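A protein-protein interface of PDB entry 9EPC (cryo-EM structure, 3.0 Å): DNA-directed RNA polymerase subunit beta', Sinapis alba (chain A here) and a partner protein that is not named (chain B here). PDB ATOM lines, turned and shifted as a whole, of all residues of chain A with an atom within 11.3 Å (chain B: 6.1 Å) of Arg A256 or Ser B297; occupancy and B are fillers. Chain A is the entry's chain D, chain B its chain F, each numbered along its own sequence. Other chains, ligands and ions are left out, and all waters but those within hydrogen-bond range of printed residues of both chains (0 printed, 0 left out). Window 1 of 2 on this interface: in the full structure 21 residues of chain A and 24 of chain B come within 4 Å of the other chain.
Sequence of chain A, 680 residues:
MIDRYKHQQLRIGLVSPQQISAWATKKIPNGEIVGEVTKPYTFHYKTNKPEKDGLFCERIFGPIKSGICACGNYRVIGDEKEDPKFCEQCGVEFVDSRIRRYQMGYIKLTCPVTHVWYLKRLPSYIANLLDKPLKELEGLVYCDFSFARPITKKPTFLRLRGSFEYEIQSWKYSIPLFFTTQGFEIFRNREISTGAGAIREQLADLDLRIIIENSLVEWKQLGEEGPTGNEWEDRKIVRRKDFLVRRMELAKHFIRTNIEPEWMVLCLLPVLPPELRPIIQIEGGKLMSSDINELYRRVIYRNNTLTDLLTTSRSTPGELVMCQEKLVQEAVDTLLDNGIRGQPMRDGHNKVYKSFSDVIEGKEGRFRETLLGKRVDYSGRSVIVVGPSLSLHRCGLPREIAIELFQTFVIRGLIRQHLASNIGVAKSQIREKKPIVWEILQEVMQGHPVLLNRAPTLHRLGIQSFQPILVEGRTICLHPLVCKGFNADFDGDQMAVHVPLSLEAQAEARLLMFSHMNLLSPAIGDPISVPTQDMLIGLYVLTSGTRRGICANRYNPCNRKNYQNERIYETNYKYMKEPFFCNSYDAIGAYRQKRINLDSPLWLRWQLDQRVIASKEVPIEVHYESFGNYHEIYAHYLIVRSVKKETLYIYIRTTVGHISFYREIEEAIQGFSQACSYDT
Among the printed residues, pairs that only touch across the chains: Lys A252 with Tyr B467 (3.2 Å), Glu A260 with Lys B455 (3.3 Å), Ile A255 with Tyr B467 (3.4 Å), Arg A256 with Ile B466 (3.5 Å), Arg A256 with Tyr B467 (3.5 Å), Thr A257 with Tyr B298 (3.6 Å), Ile A259 with Lys B455 (3.6 Å), Asn A258 with Lys B455 (3.6 Å), Ile A255 with Lys B455 (3.8 Å), Arg A256 with Tyr B298 (3.9 Å) and Arg A256 with Ala B295 (3.9 Å).
Of the printed residues of chain B, Arg A256 touches Ala B295, Ser B297, Tyr B298, Ile B466 and Tyr B467. Of chain A, only Arg A256 comes within 4 Å of Ser B297. Of chain A, only Arg A209 (2.7 Å), Lys A252 (3.2 Å), Ile A255 (3.4 Å) and Arg A256 (3.5 Å) come within 4 Å of Tyr B467. Of the printed residues of chain B, Ile A259 touches Lys B455 (3.6 Å). Of the printed residues of chain B, Lys A252 touches Tyr B467 (3.2 Å). Printed residues of chain B within 4 Å of Thr A257: Tyr B298 (3.6 Å) and Lys B455 (2.3 Å). Printed residues of chain A within 4 Å of Lys B455: Arg A209 (2.4 Å), Phe A254 (3.0 Å), Ile A255 (3.8 Å), Thr A257 (2.3 Å), Asn A258 (3.6 Å), Ile A259 (3.6 Å) and Glu A260 (3.3 Å). Arg A11 touches none of the printed residues of chain B. Leu A208 touches none of the printed residues of chain B.
Of the 20 printed residues of chain A, 9 touch a printed residue of chain B. Printed residues of chain B that touch a printed residue of chain A: Ala B295, Ser B297, Tyr B298, Lys B455, Ile B466 and Tyr B467. Hydrophobic or aromatic side chains of chain B within 4 Å of the printed part of chain A: Tyr B298, Ile B466 and Tyr B467. Among the printed residues, 16 pairs touch across the chains. Among the printed residues, no Asp or Glu carboxylate lies within 4 Å of a Lys or Arg side-chain nitrogen of the other chain.
The side-chain hydroxyl of Thr A257 sits at hydrogen-bond distance from the side-chain amide oxygen of Asn A258, 3.2 Å away. The backbone carbonyl oxygen of Tyr B298 sits at hydrogen-bond distance from the guanidinium group of Arg B300 (2.9 Å). The side-chain carboxylate of Asp B299 sits at hydrogen-bond distance from the side-chain hydroxyl of Tyr B467 (2.7 Å).
NH2 of Arg A209 lies close to O of Lys B455, 3.4 Å away. The guanidinium group (NE) of Arg A209 lies within hydrogen-bond range of the backbone carbonyl oxygen (O) of Tyr B467. O of Phe A254 lies within hydrogen-bond range of NZ of Lys B455. The guanidinium group (NH2) of Arg A256 lies close to the backbone carbonyl oxygen (O) of Ser B297 (2.4 Å). O of Thr A257 lies close to NZ of Lys B455, 2.3 Å away.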
ATOM      1  N   GLN A   9      23.964 -19.943  -1.698  1.00  0.00           N
ATOM      2  CA  GLN A   9      24.391 -19.129  -2.824  1.00  0.00           C
ATOM      3  C   GLN A   9      24.634 -17.700  -2.364  1.00  0.00           C
ATOM      4  O   GLN A   9      23.907 -17.173  -1.519  1.00  0.00           O
ATOM      5  CB  GLN A   9      23.357 -19.160  -3.949  1.00  0.00           C
ATOM      6  CG  GLN A   9      21.992 -18.633  -3.568  1.00  0.00           C
ATOM      7  CD  GLN A   9      21.012 -18.690  -4.719  1.00  0.00           C
ATOM      8  OE1 GLN A   9      21.221 -19.415  -5.690  1.00  0.00           O
ATOM      9  NE2 GLN A   9      19.935 -17.919  -4.619  1.00  0.00           N
ATOM     10  N   ARG A  11      25.173 -14.379  -4.390  1.00  0.00           N
ATOM     11  CA  ARG A  11      25.204 -13.710  -5.680  1.00  0.00           C
ATOM     12  C   ARG A  11      25.583 -12.245  -5.527  1.00  0.00           C
ATOM     13  O   ARG A  11      25.327 -11.616  -4.497  1.00  0.00           O
ATOM     14  CB  ARG A  11      23.852 -13.819  -6.386  1.00  0.00           C
ATOM     15  CG  ARG A  11      22.740 -13.010  -5.749  1.00  0.00           C
ATOM     16  CD  ARG A  11      21.464 -13.110  -6.565  1.00  0.00           C
ATOM     17  NE  ARG A  11      21.673 -12.722  -7.955  1.00  0.00           N
ATOM     18  CZ  ARG A  11      21.533 -11.487  -8.418  1.00  0.00           C
ATOM     19  NH1 ARG A  11      21.183 -10.487  -7.625  1.00  0.00           N
ATOM     20  NH2 ARG A  11      21.749 -11.249  -9.707  1.00  0.00           N
ATOM     21  N   LEU A 208      19.832  -7.342 -27.763  1.00  0.00           N
ATOM     22  CA  LEU A 208      20.856  -8.304 -27.374  1.00  0.00           C
ATOM     23  C   LEU A 208      20.791  -9.564 -28.227  1.00  0.00           C
ATOM     24  O   LEU A 208      21.826 -10.178 -28.513  1.00  0.00           O
ATOM     25  CB  LEU A 208      20.715  -8.638 -25.892  1.00  0.00           C
ATOM     26  CG  LEU A 208      20.915  -7.441 -24.963  1.00  0.00           C
ATOM     27  CD1 LEU A 208      20.689  -7.828 -23.518  1.00  0.00           C
ATOM     28  CD2 LEU A 208      22.303  -6.861 -25.146  1.00  0.00           C
ATOM     29  N   ARG A 209      19.591  -9.966 -28.645  1.00  0.00           N
ATOM     30  CA  ARG A 209      19.481 -11.081 -29.578  1.00  0.00           C
ATOM     31  C   ARG A 209      20.181 -10.766 -30.890  1.00  0.00           C
ATOM     32  O   ARG A 209      20.906 -11.605 -31.435  1.00  0.00           O
ATOM     33  CB  ARG A 209      18.013 -11.421 -29.832  1.00  0.00           C
ATOM     34  CG  ARG A 209      17.436 -12.465 -28.898  1.00  0.00           C
ATOM     35  CD  ARG A 209      16.924 -11.856 -27.613  1.00  0.00           C
ATOM     36  NE  ARG A 209      16.295 -12.861 -26.767  1.00  0.00           N
ATOM     37  CZ  ARG A 209      15.663 -12.595 -25.632  1.00  0.00           C
ATOM     38  NH1 ARG A 209      15.551 -11.359 -25.179  1.00  0.00           N
ATOM     39  NH2 ARG A 209      15.130 -13.595 -24.938  1.00  0.00           N
ATOM     40  N   ILE A 212      24.083 -10.890 -30.755  1.00  0.00           N
ATOM     41  CA  ILE A 212      24.648 -12.228 -30.883  1.00  0.00           C
ATOM     42  C   ILE A 212      24.671 -12.663 -32.342  1.00  0.00           C
ATOM     43  O   ILE A 212      25.653 -13.248 -32.815  1.00  0.00           O
ATOM     44  CB  ILE A 212      23.866 -13.222 -30.010  1.00  0.00           C
ATOM     45  CG1 ILE A 212      23.828 -12.741 -28.561  1.00  0.00           C
ATOM     46  CG2 ILE A 212      24.489 -14.601 -30.089  1.00  0.00           C
ATOM     47  CD1 ILE A 212      22.991 -13.611 -27.659  1.00  0.00           C
ATOM     48  N   MET A 248      29.711 -11.211 -27.762  1.00  0.00           N
ATOM     49  CA  MET A 248      28.560 -12.106 -27.721  1.00  0.00           C
ATOM     50  C   MET A 248      28.483 -12.844 -26.392  1.00  0.00           C
ATOM     51  O   MET A 248      27.385 -13.119 -25.894  1.00  0.00           O
ATOM     52  CB  MET A 248      28.606 -13.090 -28.889  1.00  0.00           C
ATOM     53  CG  MET A 248      29.855 -13.942 -28.956  1.00  0.00           C
ATOM     54  SD  MET A 248      29.796 -15.105 -30.330  1.00  0.00           S
ATOM     55  CE  MET A 248      28.291 -15.994 -29.945  1.00  0.00           C
ATOM     56  N   GLU A 249      29.634 -13.166 -25.798  1.00  0.00           N
ATOM     57  CA  GLU A 249      29.629 -13.769 -24.470  1.00  0.00           C
ATOM     58  C   GLU A 249      29.003 -12.828 -23.453  1.00  0.00           C
ATOM     59  O   GLU A 249      28.246 -13.261 -22.577  1.00  0.00           O
ATOM     60  CB  GLU A 249      31.050 -14.137 -24.052  1.00  0.00           C
ATOM     61  CG  GLU A 249      31.147 -14.740 -22.662  1.00  0.00           C
ATOM     62  CD  GLU A 249      32.579 -15.000 -22.236  1.00  0.00           C
ATOM     63  OE1 GLU A 249      33.501 -14.694 -23.021  1.00  0.00           O
ATOM     64  OE2 GLU A 249      32.782 -15.511 -21.115  1.00  0.00           O
ATOM     65  N   LEU A 250      29.313 -11.536 -23.551  1.00  0.00           N
ATOM     66  CA  LEU A 250      28.679 -10.557 -22.676  1.00  0.00           C
ATOM     67  C   LEU A 250      27.178 -10.500 -22.919  1.00  0.00           C
ATOM     68  O   LEU A 250      26.389 -10.447 -21.969  1.00  0.00           O
ATOM     69  CB  LEU A 250      29.316  -9.186 -22.890  1.00  0.00           C
ATOM     70  CG  LEU A 250      28.952  -8.082 -21.902  1.00  0.00           C
ATOM     71  CD1 LEU A 250      29.351  -8.477 -20.492  1.00  0.00           C
ATOM     72  CD2 LEU A 250      29.620  -6.781 -22.304  1.00  0.00           C
ATOM     73  N   ALA A 251      26.762 -10.523 -24.187  1.00  0.00           N
ATOM     74  CA  ALA A 251      25.339 -10.464 -24.501  1.00  0.00           C
ATOM     75  C   ALA A 251      24.609 -11.717 -24.033  1.00  0.00           C
ATOM     76  O   ALA A 251      23.493 -11.630 -23.511  1.00  0.00           O
ATOM     77  CB  ALA A 251      25.142 -10.261 -26.001  1.00  0.00           C
ATOM     78  N   LYS A 252      25.219 -12.891 -24.215  1.00  0.00           N
ATOM     79  CA  LYS A 252      24.563 -14.129 -23.806  1.00  0.00           C
ATOM     80  C   LYS A 252      24.335 -14.172 -22.303  1.00  0.00           C
ATOM     81  O   LYS A 252      23.380 -14.803 -21.839  1.00  0.00           O
ATOM     82  CB  LYS A 252      25.389 -15.337 -24.250  1.00  0.00           C
ATOM     83  CG  LYS A 252      25.408 -15.555 -25.752  1.00  0.00           C
ATOM     84  CD  LYS A 252      26.378 -16.654 -26.140  1.00  0.00           C
ATOM     85  CE  LYS A 252      25.877 -18.015 -25.702  1.00  0.00           C
ATOM     86  NZ  LYS A 252      24.620 -18.385 -26.409  1.00  0.00           N
ATOM     87  N   HIS A 253      25.193 -13.509 -21.528  1.00  0.00           N
ATOM     88  CA  HIS A 253      25.003 -13.484 -20.082  1.00  0.00           C
ATOM     89  C   HIS A 253      23.868 -12.551 -19.686  1.00  0.00           C
ATOM     90  O   HIS A 253      23.142 -12.827 -18.724  1.00  0.00           O
ATOM     91  CB  HIS A 253      26.301 -13.077 -19.390  1.00  0.00           C
ATOM     92  CG  HIS A 253      27.269 -14.204 -19.219  1.00  0.00           C
ATOM     93  ND1 HIS A 253      27.672 -15.004 -20.266  1.00  0.00           N
ATOM     94  CD2 HIS A 253      27.910 -14.669 -18.121  1.00  0.00           C
ATOM     95  CE1 HIS A 253      28.522 -15.912 -19.821  1.00  0.00           C
ATOM     96  NE2 HIS A 253      28.683 -15.731 -18.523  1.00  0.00           N
ATOM     97  N   PHE A 254      23.697 -11.444 -20.411  1.00  0.00           N
ATOM     98  CA  PHE A 254      22.695 -10.457 -20.022  1.00  0.00           C
ATOM     99  C   PHE A 254      21.283 -11.019 -20.112  1.00  0.00           C
ATOM    100  O   PHE A 254      20.467 -10.806 -19.209  1.00  0.00           O
ATOM    101  CB  PHE A 254      22.823  -9.206 -20.887  1.00  0.00           C
ATOM    102  CG  PHE A 254      23.791  -8.197 -20.352  1.00  0.00           C
ATOM    103  CD1 PHE A 254      23.504  -7.489 -19.201  1.00  0.00           C
ATOM    104  CD2 PHE A 254      24.981  -7.947 -21.004  1.00  0.00           C
ATOM    105  CE1 PHE A 254      24.391  -6.558 -18.706  1.00  0.00           C
ATOM    106  CE2 PHE A 254      25.871  -7.018 -20.515  1.00  0.00           C
ATOM    107  CZ  PHE A 254      25.576  -6.322 -19.365  1.00  0.00           C
ATOM    108  N   ILE A 255      20.973 -11.745 -21.187  1.00  0.00           N
ATOM    109  CA  ILE A 255      19.598 -12.190 -21.384  1.00  0.00           C
ATOM    110  C   ILE A 255      19.259 -13.422 -20.560  1.00  0.00           C
ATOM    111  O   ILE A 255      18.074 -13.743 -20.407  1.00  0.00           O
ATOM    112  CB  ILE A 255      19.311 -12.466 -22.867  1.00  0.00           C
ATOM    113  CG1 ILE A 255      19.928 -13.791 -23.300  1.00  0.00           C
ATOM    114  CG2 ILE A 255      19.854 -11.348 -23.724  1.00  0.00           C
ATOM    115  CD1 ILE A 255      19.685 -14.099 -24.751  1.00  0.00           C
ATOM    116  N   ARG A 256      20.252 -14.125 -20.029  1.00  0.00           N
ATOM    117  CA  ARG A 256      19.996 -15.262 -19.158  1.00  0.00           C
ATOM    118  C   ARG A 256      19.926 -14.871 -17.690  1.00  0.00           C
ATOM    119  O   ARG A 256      19.660 -15.733 -16.847  1.00  0.00           O
ATOM    120  CB  ARG A 256      21.065 -16.336 -19.355  1.00  0.00           C
ATOM    121  CG  ARG A 256      21.139 -16.874 -20.768  1.00  0.00           C
ATOM    122  CD  ARG A 256      19.817 -17.479 -21.214  1.00  0.00           C
ATOM    123  NE  ARG A 256      19.461 -18.667 -20.448  1.00  0.00           N
ATOM    124  CZ  ARG A 256      18.481 -18.720 -19.556  1.00  0.00           C
ATOM    125  NH1 ARG A 256      17.725 -17.667 -19.297  1.00  0.00           N
ATOM    126  NH2 ARG A 256      18.251 -19.862 -18.913  1.00  0.00           N
ATOM    127  N   THR A 257      20.159 -13.603 -17.365  1.00  0.00           N
ATOM    128  CA  THR A 257      20.061 -13.109 -16.002  1.00  0.00           C
ATOM    129  C   THR A 257      19.143 -11.897 -15.974  1.00  0.00           C
ATOM    130  O   THR A 257      18.675 -11.417 -17.009  1.00  0.00           O
ATOM    131  CB  THR A 257      21.434 -12.737 -15.430  1.00  0.00           C
ATOM    132  OG1 THR A 257      21.308 -12.465 -14.029  1.00  0.00           O
ATOM    133  CG2 THR A 257      21.975 -11.501 -16.119  1.00  0.00           C
ATOM    134  N   ASN A 258      18.891 -11.397 -14.766  1.00  0.00           N
ATOM    135  CA  ASN A 258      18.035 -10.236 -14.558  1.00  0.00           C
ATOM    136  C   ASN A 258      18.838  -8.954 -14.381  1.00  0.00           C
ATOM    137  O   ASN A 258      18.432  -8.069 -13.621  1.00  0.00           O
ATOM    138  CB  ASN A 258      17.124 -10.462 -13.354  1.00  0.00           C
ATOM    139  CG  ASN A 258      17.896 -10.796 -12.097  1.00  0.00           C
ATOM    140  OD1 ASN A 258      18.967 -11.400 -12.156  1.00  0.00           O
ATOM    141  ND2 ASN A 258      17.359 -10.401 -10.950  1.00  0.00           N
ATOM    142  N   ILE A 259      19.972  -8.838 -15.064  1.00  0.00           N
ATOM    143  CA  ILE A 259      20.820  -7.657 -14.990  1.00  0.00           C
ATOM    144  C   ILE A 259      20.634  -6.859 -16.271  1.00  0.00           C
ATOM    145  O   ILE A 259      20.910  -7.358 -17.368  1.00  0.00           O
ATOM    146  CB  ILE A 259      22.295  -8.034 -14.787  1.00  0.00           C
ATOM    147  CG1 ILE A 259      22.466  -8.835 -13.497  1.00  0.00           C
ATOM    148  CG2 ILE A 259      23.158  -6.787 -14.758  1.00  0.00           C
ATOM    149  CD1 ILE A 259      22.065  -8.078 -12.253  1.00  0.00           C
ATOM    150  N   GLU A 260      20.167  -5.638 -16.136  1.00  0.00           N
ATOM    151  CA  GLU A 260      19.963  -4.787 -17.302  1.00  0.00           C
ATOM    152  C   GLU A 260      21.243  -4.030 -17.626  1.00  0.00           C
ATOM    153  O   GLU A 260      21.875  -3.479 -16.717  1.00  0.00           O
ATOM    154  CB  GLU A 260      18.831  -3.801 -17.061  1.00  0.00           C
ATOM    155  CG  GLU A 260      17.487  -4.452 -16.798  1.00  0.00           C
ATOM    156  CD  GLU A 260      16.913  -5.124 -18.029  1.00  0.00           C
ATOM    157  OE1 GLU A 260      17.353  -4.797 -19.150  1.00  0.00           O
ATOM    158  OE2 GLU A 260      16.017  -5.980 -17.874  1.00  0.00           O
ATOM    159  N   PRO A 261      21.656  -3.983 -18.894  1.00  0.00           N
ATOM    160  CA  PRO A 261      22.865  -3.221 -19.243  1.00  0.00           C
ATOM    161  C   PRO A 261      22.754  -1.736 -18.962  1.00  0.00           C
ATOM    162  O   PRO A 261      23.788  -1.070 -18.835  1.00  0.00           O
ATOM    163  CB  PRO A 261      23.030  -3.497 -20.743  1.00  0.00           C
ATOM    164  CG  PRO A 261      21.668  -3.887 -21.209  1.00  0.00           C
ATOM    165  CD  PRO A 261      21.052  -4.631 -20.068  1.00  0.00           C
ATOM    166  N   TRP A 263      22.056  -0.472 -16.283  1.00  0.00           N
ATOM    167  CA  TRP A 263      22.525  -0.241 -14.926  1.00  0.00           C
ATOM    168  C   TRP A 263      24.005   0.114 -14.881  1.00  0.00           C
ATOM    169  O   TRP A 263      24.475   0.622 -13.859  1.00  0.00           O
ATOM    170  CB  TRP A 263      22.242  -1.471 -14.065  1.00  0.00           C
ATOM    171  CG  TRP A 263      20.793  -1.876 -14.062  1.00  0.00           C
ATOM    172  CD1 TRP A 263      19.744  -1.177 -14.582  1.00  0.00           C
ATOM    173  CD2 TRP A 263      20.241  -3.075 -13.513  1.00  0.00           C
ATOM    174  NE1 TRP A 263      18.574  -1.865 -14.392  1.00  0.00           N
ATOM    175  CE2 TRP A 263      18.853  -3.035 -13.735  1.00  0.00           C
ATOM    176  CE3 TRP A 263      20.784  -4.177 -12.852  1.00  0.00           C
ATOM    177  CZ2 TRP A 263      18.003  -4.055 -13.326  1.00  0.00           C
ATOM    178  CZ3 TRP A 263      19.939  -5.187 -12.444  1.00  0.00           C
ATOM    179  CH2 TRP A 263      18.564  -5.118 -12.681  1.00  0.00           C
ATOM    180  N   GLY B 259      13.856 -26.204  -9.808  1.00  0.00           N
ATOM    181  CA  GLY B 259      14.404 -25.116 -10.586  1.00  0.00           C
ATOM    182  C   GLY B 259      15.832 -24.749 -10.256  1.00  0.00           C
ATOM    183  O   GLY B 259      16.380 -23.836 -10.888  1.00  0.00           O
ATOM    184  N   PRO B 261      19.347 -26.522 -10.326  1.00  0.00           N
ATOM    185  CA  PRO B 261      20.085 -27.751 -10.660  1.00  0.00           C
ATOM    186  C   PRO B 261      21.138 -28.129  -9.635  1.00  0.00           C
ATOM    187  O   PRO B 261      21.435 -29.320  -9.480  1.00  0.00           O
ATOM    188  CB  PRO B 261      20.714 -27.418 -12.019  1.00  0.00           C
ATOM    189  CG  PRO B 261      19.868 -26.321 -12.572  1.00  0.00           C
ATOM    190  CD  PRO B 261      19.455 -25.509 -11.388  1.00  0.00           C
ATOM    191  N   ALA B 295      15.826 -25.240 -16.293  1.00  0.00           N
ATOM    192  CA  ALA B 295      16.389 -24.263 -15.375  1.00  0.00           C
ATOM    193  C   ALA B 295      15.956 -22.859 -15.772  1.00  0.00           C
ATOM    194  O   ALA B 295      16.047 -22.474 -16.942  1.00  0.00           O
ATOM    195  CB  ALA B 295      17.915 -24.352 -15.351  1.00  0.00           C
ATOM    196  N   ASP B 296      15.490 -22.098 -14.785  1.00  0.00           N
ATOM    197  CA  ASP B 296      15.082 -20.713 -14.972  1.00  0.00           C
ATOM    198  C   ASP B 296      16.218 -19.743 -14.680  1.00  0.00           C
ATOM    199  O   ASP B 296      15.975 -18.631 -14.203  1.00  0.00           O
ATOM    200  CB  ASP B 296      13.877 -20.400 -14.087  1.00  0.00           C
ATOM    201  CG  ASP B 296      14.100 -20.802 -12.643  1.00  0.00           C
ATOM    202  OD1 ASP B 296      14.741 -20.028 -11.901  1.00  0.00           O
ATOM    203  OD2 ASP B 296      13.644 -21.896 -12.253  1.00  0.00           O
ATOM    204  N   SER B 297      17.454 -20.146 -14.964  1.00  0.00           N
ATOM    205  CA  SER B 297      18.634 -19.407 -14.542  1.00  0.00           C
ATOM    206  C   SER B 297      19.685 -19.398 -15.642  1.00  0.00           C
ATOM    207  O   SER B 297      19.376 -19.660 -16.809  1.00  0.00           O
ATOM    208  CB  SER B 297      19.208 -20.003 -13.258  1.00  0.00           C
ATOM    209  OG  SER B 297      18.263 -19.942 -12.203  1.00  0.00           O
ATOM    210  N   TYR B 298      20.923 -19.083 -15.274  1.00  0.00           N
ATOM    211  CA  TYR B 298      22.025 -18.893 -16.203  1.00  0.00           C
ATOM    212  C   TYR B 298      22.236 -20.134 -17.072  1.00  0.00           C
ATOM    213  O   TYR B 298      21.667 -21.201 -16.833  1.00  0.00           O
ATOM    214  CB  TYR B 298      23.297 -18.551 -15.433  1.00  0.00           C
ATOM    215  CG  TYR B 298      23.037 -17.739 -14.188  1.00  0.00           C
ATOM    216  CD1 TYR B 298      22.946 -16.358 -14.244  1.00  0.00           C
ATOM    217  CD2 TYR B 298      22.876 -18.356 -12.957  1.00  0.00           C
ATOM    218  CE1 TYR B 298      22.704 -15.613 -13.110  1.00  0.00           C
ATOM    219  CE2 TYR B 298      22.632 -17.620 -11.820  1.00  0.00           C
ATOM    220  CZ  TYR B 298      22.549 -16.249 -11.901  1.00  0.00           C
ATOM    221  OH  TYR B 298      22.309 -15.509 -10.768  1.00  0.00           O
ATOM    222  N   ASP B 299      23.072 -19.977 -18.095  1.00  0.00           N
ATOM    223  CA  ASP B 299      23.286 -21.029 -19.080  1.00  0.00           C
ATOM    224  C   ASP B 299      23.774 -22.313 -18.420  1.00  0.00           C
ATOM    225  O   ASP B 299      24.681 -22.297 -17.585  1.00  0.00           O
ATOM    226  CB  ASP B 299      24.294 -20.555 -20.129  1.00  0.00           C
ATOM    227  CG  ASP B 299      24.698 -21.648 -21.099  1.00  0.00           C
ATOM    228  OD1 ASP B 299      25.463 -22.552 -20.704  1.00  0.00           O
ATOM    229  OD2 ASP B 299      24.248 -21.602 -22.263  1.00  0.00           O
ATOM    230  N   ARG B 300      23.168 -23.435 -18.815  1.00  0.00           N
ATOM    231  CA  ARG B 300      23.512 -24.737 -18.259  1.00  0.00           C
ATOM    232  C   ARG B 300      23.902 -25.752 -19.327  1.00  0.00           C
ATOM    233  O   ARG B 300      24.016 -26.941 -19.014  1.00  0.00           O
ATOM    234  CB  ARG B 300      22.349 -25.300 -17.434  1.00  0.00           C
ATOM    235  CG  ARG B 300      21.797 -24.353 -16.392  1.00  0.00           C
ATOM    236  CD  ARG B 300      22.880 -23.868 -15.451  1.00  0.00           C
ATOM    237  NE  ARG B 300      22.377 -22.859 -14.527  1.00  0.00           N
ATOM    238  CZ  ARG B 300      22.141 -23.075 -13.242  1.00  0.00           C
ATOM    239  NH1 ARG B 300      22.379 -24.250 -12.683  1.00  0.00           N
ATOM    240  NH2 ARG B 300      21.662 -22.085 -12.495  1.00  0.00           N
ATOM    241  N   TYR B 335      19.062 -24.650 -26.538  1.00  0.00           N
ATOM    242  CA  TYR B 335      20.304 -23.891 -26.588  1.00  0.00           C
ATOM    243  C   TYR B 335      20.819 -23.692 -28.008  1.00  0.00           C
ATOM    244  O   TYR B 335      21.990 -23.345 -28.185  1.00  0.00           O
ATOM    245  CB  TYR B 335      21.373 -24.572 -25.732  1.00  0.00           C
ATOM    246  CG  TYR B 335      21.175 -24.363 -24.250  1.00  0.00           C
ATOM    247  CD1 TYR B 335      21.519 -23.162 -23.649  1.00  0.00           C
ATOM    248  CD2 TYR B 335      20.644 -25.365 -23.451  1.00  0.00           C
ATOM    249  CE1 TYR B 335      21.340 -22.963 -22.298  1.00  0.00           C
ATOM    250  CE2 TYR B 335      20.463 -25.174 -22.097  1.00  0.00           C
ATOM    251  CZ  TYR B 335      20.815 -23.971 -21.525  1.00  0.00           C
ATOM    252  OH  TYR B 335      20.634 -23.775 -20.177  1.00  0.00           O
ATOM    253  N   LYS B 455      14.105  -7.285 -22.508  1.00  0.00           N
ATOM    254  CA  LYS B 455      14.738  -8.541 -22.881  1.00  0.00           C
ATOM    255  C   LYS B 455      13.729  -9.610 -23.284  1.00  0.00           C
ATOM    256  O   LYS B 455      14.093 -10.786 -23.393  1.00  0.00           O
ATOM    257  CB  LYS B 455      15.625  -9.034 -21.739  1.00  0.00           C
ATOM    258  CG  LYS B 455      16.857  -8.169 -21.520  1.00  0.00           C
ATOM    259  CD  LYS B 455      17.266  -8.123 -20.059  1.00  0.00           C
ATOM    260  CE  LYS B 455      17.566  -9.506 -19.519  1.00  0.00           C
ATOM    261  NZ  LYS B 455      18.049  -9.449 -18.113  1.00  0.00           N
ATOM    262  N   ILE B 466      15.578 -19.990 -25.431  1.00  0.00           N
ATOM    263  CA  ILE B 466      16.463 -19.646 -24.311  1.00  0.00           C
ATOM    264  C   ILE B 466      17.197 -18.366 -24.689  1.00  0.00           C
ATOM    265  O   ILE B 466      17.171 -17.381 -23.944  1.00  0.00           O
ATOM    266  CB  ILE B 466      17.463 -20.754 -23.918  1.00  0.00           C
ATOM    267  CG1 ILE B 466      16.911 -21.563 -22.745  1.00  0.00           C
ATOM    268  CG2 ILE B 466      18.784 -20.169 -23.481  1.00  0.00           C
ATOM    269  CD1 ILE B 466      17.779 -22.723 -22.349  1.00  0.00           C
ATOM    270  N   TYR B 467      17.856 -18.369 -25.849  1.00  0.00           N
ATOM    271  CA  TYR B 467      18.495 -17.168 -26.377  1.00  0.00           C
ATOM    272  C   TYR B 467      17.651 -16.525 -27.471  1.00  0.00           C
ATOM    273  O   TYR B 467      17.234 -15.370 -27.343  1.00  0.00           O
ATOM    274  CB  TYR B 467      19.894 -17.496 -26.914  1.00  0.00           C
ATOM    275  CG  TYR B 467      20.882 -17.923 -25.855  1.00  0.00           C
ATOM    276  CD1 TYR B 467      21.468 -16.993 -25.011  1.00  0.00           C
ATOM    277  CD2 TYR B 467      21.241 -19.254 -25.709  1.00  0.00           C
ATOM    278  CE1 TYR B 467      22.370 -17.374 -24.045  1.00  0.00           C
ATOM    279  CE2 TYR B 467      22.145 -19.646 -24.743  1.00  0.00           C
ATOM    280  CZ  TYR B 467      22.706 -18.701 -23.914  1.00  0.00           C
ATOM    281  OH  TYR B 467      23.609 -19.083 -22.951  1.00  0.00           O
